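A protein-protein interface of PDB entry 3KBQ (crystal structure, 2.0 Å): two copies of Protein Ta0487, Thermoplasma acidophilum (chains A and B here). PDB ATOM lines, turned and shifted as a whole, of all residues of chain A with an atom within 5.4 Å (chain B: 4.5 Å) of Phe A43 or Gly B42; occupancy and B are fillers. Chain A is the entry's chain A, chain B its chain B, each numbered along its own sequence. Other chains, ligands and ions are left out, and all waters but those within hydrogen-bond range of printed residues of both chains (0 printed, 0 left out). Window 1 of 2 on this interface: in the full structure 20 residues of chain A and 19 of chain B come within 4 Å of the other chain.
C of Arg B41 touches CD2 of Leu A16, at 3.7 Å.
Leu A16 touches Gly B42.
Arg A41 touches Val B44 (CA to O, 3.5 Å).
CA of Phe B43 touches O of Gly A42, at 3.5 Å.
Gly B42 touches Phe A43.
Trp B54 touches Phe A43 (CH2 to CE1, 3.6 Å).
Arg B41 touches Val A44.
Trp A54 touches Arg B41.
CH2 of Trp A54 touches CE1 of Phe B43, at 3.8 Å.
Val A58 touches Trp B54.
The backbone NH of Val A44 lies within hydrogen-bond range of the backbone carbonyl oxygen of Gly B42 (2.8 Å).
O of Gly A42 sits at hydrogen-bond distance from N of Val B44, 2.7 Å away.
Arg A41 touches Val B44, and with the chains exchanged Val A44 touches Arg B41.
Gly A42 touches Phe B43, and with the chains exchanged Phe A43 touches Gly B42.
Gly A42 touches Val B44, and with the chains exchanged Val A44 touches Gly B42.
Phe A43 touches Trp B54, and with the chains exchanged Trp A54 touches Phe B43.
Printed residues of chain B that touch a printed residue of chain A: Arg B41, Gly B42, Phe B43, Val B44 and Trp B54.
Of the 15 printed residues of chain A, 7 touch a printed residue of chain B.
Among the printed residues, 13 pairs touch across the chains.
O of Val B8 lies within hydrogen-bond range of N of Phe B43.
N of Val B8 is in hydrogen-bond range of O of Arg B41 (3.1 Å).
The backbone carbonyl oxygen of Arg A41 is in hydrogen-bond range of the backbone NH of Val A8 (2.9 Å).
The backbone carbonyl oxygen of Phe A43 sits at hydrogen-bond distance from the backbone NH of Thr A10 (2.8 Å).
O of Val A8 lies within hydrogen-bond range of N of Phe A43 (3.0 Å).
Of chain B, only Gly B42 (3.6 Å) and Trp B54 (3.6 Å) come within 4 Å of Phe A43.
Of the printed residues of chain A, Gly B42 touches Leu A16 (3.5 Å), Phe A43 (3.6 Å) and Val A44 (2.8 Å).
Printed residues of chain B within 4 Å of Trp A54: Arg B41 and Phe B43.
Of the printed residues of chain B, Leu A16 touches Arg B41 (3.7 Å) and Gly B42 (3.5 Å).
Of the printed residues of chain B, Val A58 touches Trp B54 (3.9 Å).
Of the printed residues of chain B, Arg A41 touches Val B44 (3.5 Å) and Trp B54 (3.2 Å).
Ala A59 touches none of the printed residues of chain B.
The nearest printed residue of chain B that does not touch Phe A43 is Val B44 (4.9 Å).
The nearest printed residue of chain A that does not touch Gly B42 is Gly A42 (4.02 Å).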
ATOM      1  N   SER A   7      23.619 -17.160 -16.859  1.00  0.00           N
ATOM      2  CA  SER A   7      24.377 -15.986 -17.298  1.00  0.00           C
ATOM      3  C   SER A   7      25.651 -15.967 -16.556  1.00  0.00           C
ATOM      4  O   SER A   7      25.692 -16.455 -15.434  1.00  0.00           O
ATOM      5  CB  SER A   7      23.624 -14.686 -17.028  1.00  0.00           C
ATOM      6  OG  SER A   7      22.823 -14.511 -18.167  1.00  0.00           O
ATOM      7  N   VAL A   8      26.679 -15.340 -17.130  1.00  0.00           N
ATOM      8  CA  VAL A   8      27.984 -15.314 -16.459  1.00  0.00           C
ATOM      9  C   VAL A   8      28.368 -13.845 -16.166  1.00  0.00           C
ATOM     10  O   VAL A   8      28.153 -12.987 -17.013  1.00  0.00           O
ATOM     11  CB  VAL A   8      29.024 -16.014 -17.363  1.00  0.00           C
ATOM     12  CG1 VAL A   8      30.443 -15.904 -16.772  1.00  0.00           C
ATOM     13  CG2 VAL A   8      28.631 -17.463 -17.560  1.00  0.00           C
ATOM     14  N   ILE A   9      28.894 -13.539 -14.967  1.00  0.00           N
ATOM     15  CA  ILE A   9      29.353 -12.198 -14.700  1.00  0.00           C
ATOM     16  C   ILE A   9      30.862 -12.273 -14.406  1.00  0.00           C
ATOM     17  O   ILE A   9      31.303 -13.129 -13.626  1.00  0.00           O
ATOM     18  CB  ILE A   9      28.556 -11.536 -13.522  1.00  0.00           C
ATOM     19  CG1 ILE A   9      27.050 -11.405 -13.880  1.00  0.00           C
ATOM     20  CG2 ILE A   9      29.194 -10.156 -13.083  1.00  0.00           C
ATOM     21  CD1 ILE A   9      26.112 -11.107 -12.620  1.00  0.00           C
ATOM     22  N   THR A  10      31.636 -11.357 -14.985  1.00  0.00           N
ATOM     23  CA  THR A  10      33.035 -11.214 -14.649  1.00  0.00           C
ATOM     24  C   THR A  10      33.252  -9.846 -14.045  1.00  0.00           C
ATOM     25  O   THR A  10      32.825  -8.836 -14.625  1.00  0.00           O
ATOM     26  CB  THR A  10      33.987 -11.447 -15.883  1.00  0.00           C
ATOM     27  OG1 THR A  10      33.646 -12.703 -16.473  1.00  0.00           O
ATOM     28  CG2 THR A  10      35.453 -11.530 -15.423  1.00  0.00           C
ATOM     29  N   LEU A  16      38.312  -5.866 -18.223  1.00  0.00           N
ATOM     30  CA  LEU A  16      37.854  -4.796 -19.131  1.00  0.00           C
ATOM     31  C   LEU A  16      38.990  -4.123 -19.860  1.00  0.00           C
ATOM     32  O   LEU A  16      38.838  -3.773 -21.042  1.00  0.00           O
ATOM     33  CB  LEU A  16      37.135  -3.710 -18.334  1.00  0.00           C
ATOM     34  CG  LEU A  16      35.821  -4.262 -17.778  1.00  0.00           C
ATOM     35  CD1 LEU A  16      35.394  -3.355 -16.617  1.00  0.00           C
ATOM     36  CD2 LEU A  16      34.720  -4.310 -18.860  1.00  0.00           C
ATOM     37  N   ARG A  41      24.105 -14.892 -21.630  1.00  0.00           N
ATOM     38  CA  ARG A  41      24.773 -13.589 -21.669  1.00  0.00           C
ATOM     39  C   ARG A  41      26.032 -13.567 -20.841  1.00  0.00           C
ATOM     40  O   ARG A  41      26.156 -14.310 -19.838  1.00  0.00           O
ATOM     41  CB  ARG A  41      23.870 -12.471 -21.099  1.00  0.00           C
ATOM     42  CG  ARG A  41      22.849 -12.039 -22.064  1.00  0.00           C
ATOM     43  CD  ARG A  41      22.026 -10.833 -21.514  1.00  0.00           C
ATOM     44  NE  ARG A  41      20.837 -10.661 -22.338  1.00  0.00           N
ATOM     45  CZ  ARG A  41      19.902  -9.753 -22.120  1.00  0.00           C
ATOM     46  NH1 ARG A  41      20.022  -8.927 -21.076  1.00  0.00           N
ATOM     47  NH2 ARG A  41      18.837  -9.696 -22.931  1.00  0.00           N
ATOM     48  N   GLY A  42      26.949 -12.687 -21.212  1.00  0.00           N
ATOM     49  CA  GLY A  42      28.152 -12.508 -20.388  1.00  0.00           C
ATOM     50  C   GLY A  42      28.236 -11.017 -20.120  1.00  0.00           C
ATOM     51  O   GLY A  42      28.082 -10.218 -21.054  1.00  0.00           O
ATOM     52  N   PHE A  43      28.449 -10.648 -18.860  1.00  0.00           N
ATOM     53  CA  PHE A  43      28.587  -9.256 -18.427  1.00  0.00           C
ATOM     54  C   PHE A  43      29.988  -9.105 -17.883  1.00  0.00           C
ATOM     55  O   PHE A  43      30.447  -9.944 -17.114  1.00  0.00           O
ATOM     56  CB  PHE A  43      27.652  -8.957 -17.259  1.00  0.00           C
ATOM     57  CG  PHE A  43      26.175  -9.214 -17.536  1.00  0.00           C
ATOM     58  CD1 PHE A  43      25.325  -8.134 -17.733  1.00  0.00           C
ATOM     59  CD2 PHE A  43      25.649 -10.499 -17.534  1.00  0.00           C
ATOM     60  CE1 PHE A  43      23.952  -8.329 -17.971  1.00  0.00           C
ATOM     61  CE2 PHE A  43      24.300 -10.730 -17.782  1.00  0.00           C
ATOM     62  CZ  PHE A  43      23.414  -9.647 -17.997  1.00  0.00           C
ATOM     63  N   VAL A  44      30.688  -8.037 -18.246  1.00  0.00           N
ATOM     64  CA  VAL A  44      31.946  -7.806 -17.622  1.00  0.00           C
ATOM     65  C   VAL A  44      31.815  -6.409 -16.990  1.00  0.00           C
ATOM     66  O   VAL A  44      31.450  -5.479 -17.682  1.00  0.00           O
ATOM     67  CB  VAL A  44      33.152  -7.855 -18.622  1.00  0.00           C
ATOM     68  CG1 VAL A  44      34.428  -7.660 -17.848  1.00  0.00           C
ATOM     69  CG2 VAL A  44      33.251  -9.198 -19.285  1.00  0.00           C
ATOM     70  N   VAL A  45      32.064  -6.278 -15.690  1.00  0.00           N
ATOM     71  CA  VAL A  45      31.888  -4.980 -15.030  1.00  0.00           C
ATOM     72  C   VAL A  45      33.070  -4.621 -14.182  1.00  0.00           C
ATOM     73  O   VAL A  45      33.915  -5.487 -13.837  1.00  0.00           O
ATOM     74  CB  VAL A  45      30.566  -4.892 -14.127  1.00  0.00           C
ATOM     75  CG1 VAL A  45      29.329  -4.853 -15.026  1.00  0.00           C
ATOM     76  CG2 VAL A  45      30.513  -6.057 -13.092  1.00  0.00           C
ATOM     77  N   TRP A  54      23.896  -3.784 -10.854  1.00  0.00           N
ATOM     78  CA  TRP A  54      23.157  -3.731 -12.095  1.00  0.00           C
ATOM     79  C   TRP A  54      23.273  -5.062 -12.883  1.00  0.00           C
ATOM     80  O   TRP A  54      22.260  -5.572 -13.393  1.00  0.00           O
ATOM     81  CB  TRP A  54      23.605  -2.552 -12.968  1.00  0.00           C
ATOM     82  CG  TRP A  54      23.168  -2.763 -14.404  1.00  0.00           C
ATOM     83  CD1 TRP A  54      21.949  -2.463 -14.928  1.00  0.00           C
ATOM     84  CD2 TRP A  54      23.927  -3.361 -15.454  1.00  0.00           C
ATOM     85  NE1 TRP A  54      21.895  -2.855 -16.242  1.00  0.00           N
ATOM     86  CE2 TRP A  54      23.104  -3.382 -16.602  1.00  0.00           C
ATOM     87  CE3 TRP A  54      25.233  -3.885 -15.540  1.00  0.00           C
ATOM     88  CZ2 TRP A  54      23.514  -3.943 -17.812  1.00  0.00           C
ATOM     89  CZ3 TRP A  54      25.657  -4.437 -16.738  1.00  0.00           C
ATOM     90  CH2 TRP A  54      24.799  -4.449 -17.878  1.00  0.00           C
ATOM     91  N   ALA A  55      24.488  -5.605 -12.993  1.00  0.00           N
ATOM     92  CA  ALA A  55      24.703  -6.882 -13.679  1.00  0.00           C
ATOM     93  C   ALA A  55      23.958  -8.030 -13.020  1.00  0.00           C
ATOM     94  O   ALA A  55      23.289  -8.809 -13.714  1.00  0.00           O
ATOM     95  CB  ALA A  55      26.169  -7.211 -13.841  1.00  0.00           C
ATOM     96  N   VAL A  58      20.100  -7.554 -13.973  1.00  0.00           N
ATOM     97  CA  VAL A  58      19.779  -8.003 -15.346  1.00  0.00           C
ATOM     98  C   VAL A  58      20.013  -9.527 -15.532  1.00  0.00           C
ATOM     99  O   VAL A  58      19.152 -10.222 -16.102  1.00  0.00           O
ATOM    100  CB  VAL A  58      20.556  -7.198 -16.428  1.00  0.00           C
ATOM    101  CG1 VAL A  58      20.090  -7.650 -17.829  1.00  0.00           C
ATOM    102  CG2 VAL A  58      20.281  -5.669 -16.238  1.00  0.00           C
ATOM    103  N   ALA A  59      21.145 -10.043 -15.044  1.00  0.00           N
ATOM    104  CA  ALA A  59      21.429 -11.505 -15.142  1.00  0.00           C
ATOM    105  C   ALA A  59      20.260 -12.306 -14.563  1.00  0.00           C
ATOM    106  O   ALA A  59      19.810 -13.260 -15.175  1.00  0.00           O
ATOM    107  CB  ALA A  59      22.741 -11.886 -14.438  1.00  0.00           C
ATOM    108  N   VAL A  62      17.148 -12.657 -16.802  1.00  0.00           N
ATOM    109  CA  VAL A  62      17.167 -13.408 -18.027  1.00  0.00           C
ATOM    110  C   VAL A  62      17.631 -14.868 -17.798  1.00  0.00           C
ATOM    111  O   VAL A  62      17.706 -15.663 -18.740  1.00  0.00           O
ATOM    112  CB  VAL A  62      18.029 -12.639 -19.117  1.00  0.00           C
ATOM    113  CG1 VAL A  62      17.416 -11.253 -19.373  1.00  0.00           C
ATOM    114  CG2 VAL A  62      19.508 -12.510 -18.672  1.00  0.00           C
ATOM    115  N   VAL B   8      32.608  -2.402 -24.729  1.00  0.00           N
ATOM    116  CA  VAL B   8      32.988  -3.437 -25.663  1.00  0.00           C
ATOM    117  C   VAL B   8      31.864  -4.476 -25.731  1.00  0.00           C
ATOM    118  O   VAL B   8      31.327  -4.914 -24.732  1.00  0.00           O
ATOM    119  CB  VAL B   8      34.323  -4.068 -25.244  1.00  0.00           C
ATOM    120  CG1 VAL B   8      34.828  -5.113 -26.258  1.00  0.00           C
ATOM    121  CG2 VAL B   8      35.364  -2.943 -25.041  1.00  0.00           C
ATOM    122  N   ARG B  41      32.047  -1.179 -19.456  1.00  0.00           N
ATOM    123  CA  ARG B  41      31.337  -2.466 -19.392  1.00  0.00           C
ATOM    124  C   ARG B  41      31.692  -3.261 -20.615  1.00  0.00           C
ATOM    125  O   ARG B  41      31.936  -2.667 -21.696  1.00  0.00           O
ATOM    126  CB  ARG B  41      29.811  -2.277 -19.371  1.00  0.00           C
ATOM    127  CG  ARG B  41      29.289  -1.635 -18.086  1.00  0.00           C
ATOM    128  CD  ARG B  41      27.789  -1.596 -18.123  1.00  0.00           C
ATOM    129  NE  ARG B  41      27.300  -0.878 -16.969  1.00  0.00           N
ATOM    130  CZ  ARG B  41      26.021  -0.559 -16.787  1.00  0.00           C
ATOM    131  NH1 ARG B  41      25.109  -0.949 -17.684  1.00  0.00           N
ATOM    132  NH2 ARG B  41      25.657   0.119 -15.699  1.00  0.00           N
ATOM    133  N   GLY B  42      31.675  -4.595 -20.463  1.00  0.00           N
ATOM    134  CA  GLY B  42      31.875  -5.550 -21.578  1.00  0.00           C
ATOM    135  C   GLY B  42      30.606  -6.395 -21.645  1.00  0.00           C
ATOM    136  O   GLY B  42      29.979  -6.704 -20.600  1.00  0.00           O
ATOM    137  N   PHE B  43      30.157  -6.700 -22.854  1.00  0.00           N
ATOM    138  CA  PHE B  43      28.941  -7.493 -23.044  1.00  0.00           C
ATOM    139  C   PHE B  43      29.299  -8.642 -23.967  1.00  0.00           C
ATOM    140  O   PHE B  43      30.034  -8.455 -24.951  1.00  0.00           O
ATOM    141  CB  PHE B  43      27.861  -6.660 -23.743  1.00  0.00           C
ATOM    142  CG  PHE B  43      27.513  -5.403 -23.032  1.00  0.00           C
ATOM    143  CD1 PHE B  43      26.457  -5.382 -22.158  1.00  0.00           C
ATOM    144  CD2 PHE B  43      28.264  -4.221 -23.262  1.00  0.00           C
ATOM    145  CE1 PHE B  43      26.117  -4.175 -21.478  1.00  0.00           C
ATOM    146  CE2 PHE B  43      27.958  -3.054 -22.632  1.00  0.00           C
ATOM    147  CZ  PHE B  43      26.865  -3.013 -21.714  1.00  0.00           C
ATOM    148  N   VAL B  44      28.808  -9.821 -23.649  1.00  0.00           N
ATOM    149  CA  VAL B  44      28.921 -10.947 -24.568  1.00  0.00           C
ATOM    150  C   VAL B  44      27.512 -11.436 -24.803  1.00  0.00           C
ATOM    151  O   VAL B  44      26.764 -11.752 -23.871  1.00  0.00           O
ATOM    152  CB  VAL B  44      29.813 -12.080 -24.033  1.00  0.00           C
ATOM    153  CG1 VAL B  44      30.042 -13.120 -25.145  1.00  0.00           C
ATOM    154  CG2 VAL B  44      31.171 -11.506 -23.527  1.00  0.00           C
ATOM    155  N   TRP B  54      19.910  -5.323 -27.476  1.00  0.00           N
ATOM    156  CA  TRP B  54      20.038  -5.058 -26.041  1.00  0.00           C
ATOM    157  C   TRP B  54      21.443  -4.524 -25.689  1.00  0.00           C
ATOM    158  O   TRP B  54      21.559  -3.502 -25.039  1.00  0.00           O
ATOM    159  CB  TRP B  54      19.605  -6.267 -25.159  1.00  0.00           C
ATOM    160  CG  TRP B  54      19.983  -6.076 -23.729  1.00  0.00           C
ATOM    161  CD1 TRP B  54      19.293  -5.324 -22.756  1.00  0.00           C
ATOM    162  CD2 TRP B  54      21.182  -6.537 -23.105  1.00  0.00           C
ATOM    163  NE1 TRP B  54      20.031  -5.330 -21.583  1.00  0.00           N
ATOM    164  CE2 TRP B  54      21.176  -6.064 -21.767  1.00  0.00           C
ATOM    165  CE3 TRP B  54      22.273  -7.305 -23.551  1.00  0.00           C
ATOM    166  CZ2 TRP B  54      22.222  -6.343 -20.864  1.00  0.00           C
ATOM    167  CZ3 TRP B  54      23.307  -7.608 -22.643  1.00  0.00           C
ATOM    168  CH2 TRP B  54      23.260  -7.116 -21.307  1.00  0.00           C
